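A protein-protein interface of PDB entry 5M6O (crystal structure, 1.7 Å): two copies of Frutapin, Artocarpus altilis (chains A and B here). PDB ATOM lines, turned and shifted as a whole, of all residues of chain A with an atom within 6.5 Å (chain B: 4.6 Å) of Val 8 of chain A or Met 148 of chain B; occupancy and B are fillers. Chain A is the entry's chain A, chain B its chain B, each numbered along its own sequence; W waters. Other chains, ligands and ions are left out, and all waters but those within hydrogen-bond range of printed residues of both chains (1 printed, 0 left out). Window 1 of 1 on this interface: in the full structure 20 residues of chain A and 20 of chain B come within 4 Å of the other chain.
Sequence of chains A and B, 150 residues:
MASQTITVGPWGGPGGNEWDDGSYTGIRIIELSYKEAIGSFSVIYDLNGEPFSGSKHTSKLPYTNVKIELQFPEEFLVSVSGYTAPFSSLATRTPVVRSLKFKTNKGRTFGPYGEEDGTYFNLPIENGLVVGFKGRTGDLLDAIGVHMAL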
ATOM      1  N   ILE A   6     -25.125 -18.672  14.970  1.00  0.00           N
ATOM      2  CA  ILE A   6     -25.057 -17.706  16.135  1.00  0.00           C
ATOM      3  C   ILE A   6     -23.706 -17.718  16.746  1.00  0.00           C
ATOM      4  O   ILE A   6     -23.162 -18.754  17.028  1.00  0.00           O
ATOM      5  CB  ILE A   6     -26.157 -17.957  17.145  1.00  0.00           C
ATOM      6  CG1 ILE A   6     -27.457 -17.535  16.474  1.00  0.00           C
ATOM      7  CG2 ILE A   6     -25.971 -17.096  18.382  1.00  0.00           C
ATOM      8  CD1 ILE A   6     -28.687 -18.247  16.973  1.00  0.00           C
ATOM      9  N   THR A   7     -23.028 -16.564  16.788  1.00  0.00           N
ATOM     10  CA  THR A   7     -21.767 -16.383  17.390  1.00  0.00           C
ATOM     11  C   THR A   7     -21.792 -15.287  18.495  1.00  0.00           C
ATOM     12  O   THR A   7     -22.262 -14.164  18.298  1.00  0.00           O
ATOM     13  CB  THR A   7     -20.636 -16.083  16.358  1.00  0.00           C
ATOM     14  OG1 THR A   7     -20.701 -17.126  15.331  1.00  0.00           O
ATOM     15  CG2 THR A   7     -19.446 -16.111  16.929  1.00  0.00           C
ATOM     16  N   VAL A   8     -21.324 -15.650  19.688  1.00  0.00           N
ATOM     17  CA  VAL A   8     -21.308 -14.725  20.749  1.00  0.00           C
ATOM     18  C   VAL A   8     -19.841 -14.556  21.248  1.00  0.00           C
ATOM     19  O   VAL A   8     -18.985 -15.462  21.178  1.00  0.00           O
ATOM     20  CB  VAL A   8     -22.329 -15.085  21.820  1.00  0.00           C
ATOM     21  CG1 VAL A   8     -23.807 -15.079  21.434  1.00  0.00           C
ATOM     22  CG2 VAL A   8     -21.908 -16.280  22.499  1.00  0.00           C
ATOM     23  N   GLY A   9     -19.589 -13.387  21.889  1.00  0.00           N
ATOM     24  CA  GLY A   9     -18.282 -12.906  22.219  1.00  0.00           C
ATOM     25  C   GLY A   9     -17.855 -12.002  21.109  1.00  0.00           C
ATOM     26  O   GLY A   9     -18.726 -11.562  20.309  1.00  0.00           O
ATOM     27  N   PRO A  10     -16.544 -11.830  20.942  1.00  0.00           N
ATOM     28  CA  PRO A  10     -15.499 -12.375  21.779  1.00  0.00           C
ATOM     29  C   PRO A  10     -15.332 -11.732  23.104  1.00  0.00           C
ATOM     30  O   PRO A  10     -15.717 -10.572  23.422  1.00  0.00           O
ATOM     31  CB  PRO A  10     -14.175 -12.070  21.014  1.00  0.00           C
ATOM     32  CG  PRO A  10     -14.564 -11.218  19.857  1.00  0.00           C
ATOM     33  CD  PRO A  10     -16.006 -10.759  20.058  1.00  0.00           C
ATOM     34  N   TRP A  11     -14.814 -12.504  23.991  1.00  0.00           N
ATOM     35  CA  TRP A  11     -14.295 -12.011  25.277  1.00  0.00           C
ATOM     36  C   TRP A  11     -12.784 -12.059  25.345  1.00  0.00           C
ATOM     37  O   TRP A  11     -12.102 -13.079  25.147  1.00  0.00           O
ATOM     38  CB  TRP A  11     -14.881 -12.801  26.481  1.00  0.00           C
ATOM     39  CG  TRP A  11     -16.474 -12.757  26.623  1.00  0.00           C
ATOM     40  CD1 TRP A  11     -17.246 -11.785  27.151  1.00  0.00           C
ATOM     41  CD2 TRP A  11     -17.375 -13.718  26.087  1.00  0.00           C
ATOM     42  NE1 TRP A  11     -18.547 -12.063  26.991  1.00  0.00           N
ATOM     43  CE2 TRP A  11     -18.678 -13.241  26.324  1.00  0.00           C
ATOM     44  CE3 TRP A  11     -17.199 -14.865  25.380  1.00  0.00           C
ATOM     45  CZ2 TRP A  11     -19.790 -13.951  26.003  1.00  0.00           C
ATOM     46  CZ3 TRP A  11     -18.343 -15.584  24.986  1.00  0.00           C
ATOM     47  CH2 TRP A  11     -19.595 -15.112  25.295  1.00  0.00           C
ATOM     48  N   LEU A 123     -21.540 -17.027  30.176  1.00  0.00           N
ATOM     49  CA  LEU A 123     -22.607 -17.443  29.237  1.00  0.00           C
ATOM     50  C   LEU A 123     -23.337 -18.688  29.725  1.00  0.00           C
ATOM     51  O   LEU A 123     -22.884 -19.755  29.412  1.00  0.00           O
ATOM     52  CB  LEU A 123     -21.992 -17.695  27.869  1.00  0.00           C
ATOM     53  CG  LEU A 123     -22.854 -18.072  26.650  1.00  0.00           C
ATOM     54  CD1 LEU A 123     -23.657 -16.880  26.203  1.00  0.00           C
ATOM     55  CD2 LEU A 123     -21.909 -18.669  25.613  1.00  0.00           C
ATOM     56  N   LYS A 134     -13.978 -19.909  18.605  1.00  0.00           N
ATOM     57  CA  LYS A 134     -13.049 -18.993  17.916  1.00  0.00           C
ATOM     58  C   LYS A 134     -12.265 -18.252  18.919  1.00  0.00           C
ATOM     59  O   LYS A 134     -12.714 -18.186  20.064  1.00  0.00           O
ATOM     60  CB  LYS A 134     -13.711 -18.037  16.927  1.00  0.00           C
ATOM     61  CG  LYS A 134     -14.679 -17.160  17.546  1.00  0.00           C
ATOM     62  CD  LYS A 134     -15.537 -16.397  16.517  1.00  0.00           C
ATOM     63  CE  LYS A 134     -14.723 -15.747  15.399  1.00  0.00           C
ATOM     64  NZ  LYS A 134     -15.310 -14.696  14.505  1.00  0.00           N
ATOM     65  N   ILE A 144     -11.638 -15.391  23.354  1.00  0.00           N
ATOM     66  CA  ILE A 144     -12.408 -16.582  22.966  1.00  0.00           C
ATOM     67  C   ILE A 144     -13.883 -16.170  22.744  1.00  0.00           C
ATOM     68  O   ILE A 144     -14.416 -15.250  23.337  1.00  0.00           O
ATOM     69  CB  ILE A 144     -12.274 -17.709  24.045  1.00  0.00           C
ATOM     70  CG1 ILE A 144     -12.748 -19.095  23.602  1.00  0.00           C
ATOM     71  CG2 ILE A 144     -12.979 -17.340  25.344  1.00  0.00           C
ATOM     72  CD1 ILE A 144     -13.228 -19.953  24.738  1.00  0.00           C
ATOM     73  N   GLY A 145     -14.527 -16.930  21.860  1.00  0.00           N
ATOM     74  CA  GLY A 145     -15.924 -16.724  21.511  1.00  0.00           C
ATOM     75  C   GLY A 145     -16.424 -18.145  21.142  1.00  0.00           C
ATOM     76  O   GLY A 145     -15.668 -19.088  20.916  1.00  0.00           O
ATOM     77  N   VAL A 146     -17.740 -18.209  21.054  1.00  0.00           N
ATOM     78  CA  VAL A 146     -18.457 -19.458  20.786  1.00  0.00           C
ATOM     79  C   VAL A 146     -19.546 -19.370  19.745  1.00  0.00           C
ATOM     80  O   VAL A 146     -20.415 -18.395  19.659  1.00  0.00           O
ATOM     81  CB  VAL A 146     -19.063 -20.111  22.054  1.00  0.00           C
ATOM     82  CG1 VAL A 146     -17.953 -20.410  23.048  1.00  0.00           C
ATOM     83  CG2 VAL A 146     -20.165 -19.291  22.647  1.00  0.00           C
ATOM     84  N   HIS A 147     -19.472 -20.353  18.918  1.00  0.00           N
ATOM     85  CA  HIS A 147     -20.563 -20.583  18.023  1.00  0.00           C
ATOM     86  C   HIS A 147     -21.589 -21.526  18.615  1.00  0.00           C
ATOM     87  O   HIS A 147     -21.233 -22.466  19.339  1.00  0.00           O
ATOM     88  CB  HIS A 147     -20.007 -21.309  16.825  1.00  0.00           C
ATOM     89  CG  HIS A 147     -18.922 -20.567  16.124  1.00  0.00           C
ATOM     90  ND1 HIS A 147     -19.163 -19.421  15.427  1.00  0.00           N
ATOM     91  CD2 HIS A 147     -17.689 -20.949  15.754  1.00  0.00           C
ATOM     92  CE1 HIS A 147     -18.079 -19.052  14.783  1.00  0.00           C
ATOM     93  NE2 HIS A 147     -17.149 -19.934  15.001  1.00  0.00           N
ATOM     94  N   MET A 148     -22.872 -21.204  18.375  1.00  0.00           N
ATOM     95  CA  MET A 148     -23.969 -22.029  18.998  1.00  0.00           C
ATOM     96  C   MET A 148     -25.039 -22.388  17.955  1.00  0.00           C
ATOM     97  O   MET A 148     -25.190 -21.692  16.979  1.00  0.00           O
ATOM     98  CB  MET A 148     -24.675 -21.192  20.097  1.00  0.00           C
ATOM     99  CG  MET A 148     -23.758 -20.783  21.203  1.00  0.00           C
ATOM    100  SD  MET A 148     -24.649 -19.810  22.411  1.00  0.00           S
ATOM    101  CE  MET A 148     -25.488 -21.065  23.208  1.00  0.00           C
ATOM    102  N   THR B   5     -35.892 -21.356  19.785  1.00  0.00           N
ATOM    103  CA  THR B   5     -34.679 -20.617  19.539  1.00  0.00           C
ATOM    104  C   THR B   5     -33.618 -20.892  20.615  1.00  0.00           C
ATOM    105  O   THR B   5     -33.899 -21.331  21.721  1.00  0.00           O
ATOM    106  CB  THR B   5     -35.006 -19.099  19.568  1.00  0.00           C
ATOM    107  OG1 THR B   5     -35.661 -18.744  20.795  1.00  0.00           O
ATOM    108  CG2 THR B   5     -35.985 -18.716  18.551  1.00  0.00           C
ATOM    109  N   ILE B   6     -32.408 -20.511  20.288  1.00  0.00           N
ATOM    110  CA  ILE B   6     -31.320 -20.466  21.228  1.00  0.00           C
ATOM    111  C   ILE B   6     -31.632 -19.472  22.310  1.00  0.00           C
ATOM    112  O   ILE B   6     -32.224 -18.448  22.091  1.00  0.00           O
ATOM    113  CB  ILE B   6     -30.012 -20.108  20.541  1.00  0.00           C
ATOM    114  CG1 ILE B   6     -29.560 -21.365  19.745  1.00  0.00           C
ATOM    115  CG2 ILE B   6     -28.975 -19.628  21.525  1.00  0.00           C
ATOM    116  CD1 ILE B   6     -28.334 -21.097  18.920  1.00  0.00           C
ATOM    117  N   VAL B   8     -30.094 -17.846  25.923  1.00  0.00           N
ATOM    118  CA  VAL B   8     -29.033 -17.623  26.904  1.00  0.00           C
ATOM    119  C   VAL B   8     -29.494 -16.829  28.163  1.00  0.00           C
ATOM    120  O   VAL B   8     -30.512 -16.086  28.128  1.00  0.00           O
ATOM    121  CB  VAL B   8     -27.757 -17.167  26.107  1.00  0.00           C
ATOM    122  CG1 VAL B   8     -27.397 -18.236  25.064  1.00  0.00           C
ATOM    123  CG2 VAL B   8     -27.922 -15.765  25.487  1.00  0.00           C
ATOM    124  N   LEU B 123     -23.168  -9.960  27.034  1.00  0.00           N
ATOM    125  CA  LEU B 123     -23.424 -10.787  25.842  1.00  0.00           C
ATOM    126  C   LEU B 123     -23.140  -9.971  24.533  1.00  0.00           C
ATOM    127  O   LEU B 123     -24.047  -9.336  23.989  1.00  0.00           O
ATOM    128  CB  LEU B 123     -24.916 -11.169  25.831  1.00  0.00           C
ATOM    129  CG  LEU B 123     -25.487 -12.156  24.752  1.00  0.00           C
ATOM    130  CD1 LEU B 123     -24.909 -13.494  24.982  1.00  0.00           C
ATOM    131  CD2 LEU B 123     -26.941 -12.136  24.809  1.00  0.00           C
ATOM    132  N   PRO B 124     -21.884  -9.953  24.022  1.00  0.00           N
ATOM    133  CA  PRO B 124     -21.570  -9.422  22.671  1.00  0.00           C
ATOM    134  C   PRO B 124     -22.072 -10.367  21.651  1.00  0.00           C
ATOM    135  O   PRO B 124     -21.855 -11.569  21.809  1.00  0.00           O
ATOM    136  CB  PRO B 124     -20.101  -9.351  22.619  1.00  0.00           C
ATOM    137  CG  PRO B 124     -19.637  -9.918  23.915  1.00  0.00           C
ATOM    138  CD  PRO B 124     -20.697 -10.586  24.602  1.00  0.00           C
ATOM    139  N   ILE B 125     -22.787  -9.901  20.675  1.00  0.00           N
ATOM    140  CA  ILE B 125     -23.297 -10.799  19.613  1.00  0.00           C
ATOM    141  C   ILE B 125     -22.541 -10.487  18.331  1.00  0.00           C
ATOM    142  O   ILE B 125     -22.603  -9.344  17.803  1.00  0.00           O
ATOM    143  CB  ILE B 125     -24.787 -10.671  19.418  1.00  0.00           C
ATOM    144  CG1 ILE B 125     -25.473 -10.982  20.747  1.00  0.00           C
ATOM    145  CG2 ILE B 125     -25.334 -11.653  18.313  1.00  0.00           C
ATOM    146  CD1 ILE B 125     -26.862 -10.453  20.675  1.00  0.00           C
ATOM    147  N   GLU B 126     -21.835 -11.487  17.809  1.00  0.00           N
ATOM    148  CA  GLU B 126     -21.060 -11.304  16.612  1.00  0.00           C
ATOM    149  C   GLU B 126     -21.877 -11.693  15.387  1.00  0.00           C
ATOM    150  O   GLU B 126     -21.719 -11.166  14.254  1.00  0.00           O
ATOM    151  CB  GLU B 126     -19.829 -12.126  16.731  1.00  0.00           C
ATOM    152  CG  GLU B 126     -18.687 -11.645  15.909  1.00  0.00           C
ATOM    153  CD  GLU B 126     -17.555 -12.639  15.972  1.00  0.00           C
ATOM    154  OE1 GLU B 126     -17.309 -13.202  14.870  1.00  0.00           O
ATOM    155  OE2 GLU B 126     -16.939 -12.866  17.076  1.00  0.00           O
ATOM    156  N   LEU B 129     -29.297 -12.495  15.933  1.00  0.00           N
ATOM    157  CA  LEU B 129     -30.134 -11.423  16.340  1.00  0.00           C
ATOM    158  C   LEU B 129     -30.838 -11.790  17.587  1.00  0.00           C
ATOM    159  O   LEU B 129     -31.296 -12.972  17.674  1.00  0.00           O
ATOM    160  CB  LEU B 129     -31.184 -11.184  15.224  1.00  0.00           C
ATOM    161  CG  LEU B 129     -30.769 -10.568  13.862  1.00  0.00           C
ATOM    162  CD1 LEU B 129     -31.874 -10.611  12.813  1.00  0.00           C
ATOM    163  CD2 LEU B 129     -30.126  -9.176  14.102  1.00  0.00           C
ATOM    164  N   VAL B 131     -34.178 -11.897  19.374  1.00  0.00           N
ATOM    165  CA  VAL B 131     -35.573 -12.053  18.852  1.00  0.00           C
ATOM    166  C   VAL B 131     -36.628 -12.249  19.962  1.00  0.00           C
ATOM    167  O   VAL B 131     -37.844 -12.433  19.685  1.00  0.00           O
ATOM    168  CB  VAL B 131     -35.667 -13.259  17.878  1.00  0.00           C
ATOM    169  CG1 VAL B 131     -34.864 -12.983  16.598  1.00  0.00           C
ATOM    170  CG2 VAL B 131     -35.271 -14.517  18.611  1.00  0.00           C
ATOM    171  N   VAL B 146     -32.164 -13.955  27.054  1.00  0.00           N
ATOM    172  CA  VAL B 146     -32.435 -13.603  25.684  1.00  0.00           C
ATOM    173  C   VAL B 146     -32.520 -14.762  24.790  1.00  0.00           C
ATOM    174  O   VAL B 146     -31.682 -15.628  24.785  1.00  0.00           O
ATOM    175  CB  VAL B 146     -31.418 -12.661  25.091  1.00  0.00           C
ATOM    176  CG1 VAL B 146     -31.596 -11.265  25.695  1.00  0.00           C
ATOM    177  CG2 VAL B 146     -30.008 -13.205  25.298  1.00  0.00           C
ATOM    178  N   HIS B 147     -33.486 -14.679  23.900  1.00  0.00           N
ATOM    179  CA  HIS B 147     -33.614 -15.597  22.829  1.00  0.00           C
ATOM    180  C   HIS B 147     -32.860 -15.064  21.580  1.00  0.00           C
ATOM    181  O   HIS B 147     -32.920 -13.829  21.315  1.00  0.00           O
ATOM    182  CB  HIS B 147     -35.059 -15.834  22.430  1.00  0.00           C
ATOM    183  CG  HIS B 147     -35.968 -16.322  23.541  1.00  0.00           C
ATOM    184  ND1 HIS B 147     -35.867 -17.574  24.082  1.00  0.00           N
ATOM    185  CD2 HIS B 147     -36.995 -15.740  24.173  1.00  0.00           C
ATOM    186  CE1 HIS B 147     -36.765 -17.739  25.042  1.00  0.00           C
ATOM    187  NE2 HIS B 147     -37.505 -16.660  25.075  1.00  0.00           N
ATOM    188  N   MET B 148     -32.238 -15.917  20.763  1.00  0.00           N
ATOM    189  CA  MET B 148     -31.410 -15.467  19.610  1.00  0.00           C
ATOM    190  C   MET B 148     -31.728 -16.358  18.400  1.00  0.00           C
ATOM    191  O   MET B 148     -31.952 -17.536  18.572  1.00  0.00           O
ATOM    192  CB  MET B 148     -29.939 -15.550  19.917  1.00  0.00           C
ATOM    193  CG  MET B 148     -29.489 -14.817  21.201  1.00  0.00           C
ATOM    194  SD  MET B 148     -27.745 -15.019  21.351  1.00  0.00           S
ATOM    195  CE  MET B 148     -27.321 -13.754  20.142  1.00  0.00           C
ATOM    196  N   ALA B 149     -31.690 -15.772  17.192  1.00  0.00           N
ATOM    197  CA  ALA B 149     -31.943 -16.566  15.957  1.00  0.00           C
ATOM    198  C   ALA B 149     -30.997 -15.970  14.921  1.00  0.00           C
ATOM    199  O   ALA B 149     -30.476 -14.813  15.115  1.00  0.00           O
ATOM    200  CB  ALA B 149     -33.352 -16.374  15.584  1.00  0.00           C
HETATM  201  O   HOH W   1     -14.241 -11.988  14.084  1.00  0.00           O
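The backbone carbonyl oxygen (O) of Pro 124 of chain B is in hydrogen-bond range of the backbone NH (N) of Gly 9 of chain A (2.9 Å).
N of Glu 126 of chain B sits at hydrogen-bond distance from O of Thr 7 of chain A.
The side-chain amino group (NZ) of Lys 134 of chain A is in salt-bridge range of the side-chain carboxylate (OE1) of Glu 126 of chain B (2.5 Å).
O of Lys 134 of chain A lies within hydrogen-bond range of N of Gly 145 of chain A.
The backbone NH (N) of Trp 11 of chain A lies within hydrogen-bond range of the backbone carbonyl oxygen (O) of Ile 144 of chain A.
The backbone NH of Leu 129 of chain B lies within hydrogen-bond range of the backbone carbonyl oxygen of Ala 149 of chain B (2.7 Å).
The backbone NH of Val 8 of chain A is in hydrogen-bond range of the backbone carbonyl oxygen of Val 146 of chain A (2.9 Å).
O of Ile 6 of chain A sits at hydrogen-bond distance from N of Met 148 of chain A, 2.8 Å away.
O of Ile 6 of chain B lies within hydrogen-bond range of N of Met 148 of chain B (2.9 Å).
Ile 6 of chain B touches Ile 6 of chain A (CD1 to CD1, 3.5 Å).
Met 148 of chain B touches Ile 6 of chain A.
Ala 149 of chain B touches Ile 6 of chain A.
Thr 7 of chain A touches Ile 125 of chain B (O to C, 3.7 Å).
Val 8 of chain A touches Pro 124 of chain B (CA to O, 3.4 Å).
Gly 9 of chain A touches Glu 126 of chain B (O to CB, 3.8 Å).
Pro 124 of chain B touches Trp 11 of chain A (CD to NE1, 3.5 Å).
CD1 of Leu 123 of chain A touches CD1 of Leu 123 of chain B, at 3.8 Å.
C of Met 148 of chain A touches CD1 of Ile 6 of chain B, at 3.7 Å.
Met 148 of chain A touches Val 8 of chain B.
Printed residues of chain B within 4 Å of Val 8 of chain A: Pro 124 (3.4 Å) and Met 148 (3.9 Å).
Printed residues of chain B within 4 Å of Trp 11 of chain A: Pro 124 (3.5 Å).
Val 146 of chain A touches none of the printed residues of chain B.
Printed residues of chain A within 4 Å of Ile 6 of chain B: Ile 6 (3.5 Å) and Met 148 (3.7 Å).
Printed residues of chain A within 4 Å of Met 148 of chain B: Ile 6 and Val 8.
The nearest printed residue of chain B that does not touch Val 8 of chain A is Leu 123 of chain B (4.04 Å).
The nearest printed residue of chain A that does not touch Met 148 of chain B is Thr 7 of chain A (5.4 Å).
Printed residues of chain B that touch a printed residue of chain A: Ile 6, Val 8, Leu 123, Pro 124, Ile 125, Glu 126, Met 148 and Ala 149.
Hydrophobic or aromatic side chains of chain B that line the printed part of chain A: Ile 6, Val 8, Leu 123, Pro 124, Ile 125 and Met 148.
Hydrophobic or aromatic side chains of chain A within 4 Å of the printed part of chain B: Ile 6, Val 8, Pro 10, Trp 11, Leu 123 and Met 148.
Among the printed residues, Asp or Glu carboxylates within 4 Å of a Lys or Arg side-chain nitrogen of the other chain: Lys 134 of chain A with Glu 126 of chain B (2.5 Å).
Ile 6 of chain A touches its own counterpart, Ile 6 of chain B.
Ile 6 of chain A touches Met 148 of chain B, and with the chains exchanged Met 148 of chain A touches Ile 6 of chain B.
Val 8 of chain A touches Met 148 of chain B, and with the chains exchanged Met 148 of chain A touches Val 8 of chain B.
Leu 123 of chain B touches its own counterpart, Leu 123 of chain A.
Of the 15 pairs that touch across the chains among the printed residues, 6 have their exchanged pair printed and touching as well.
Water W1 bridges NZ of Lys 134 of chain A and OE1 of Glu 126 of chain B.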
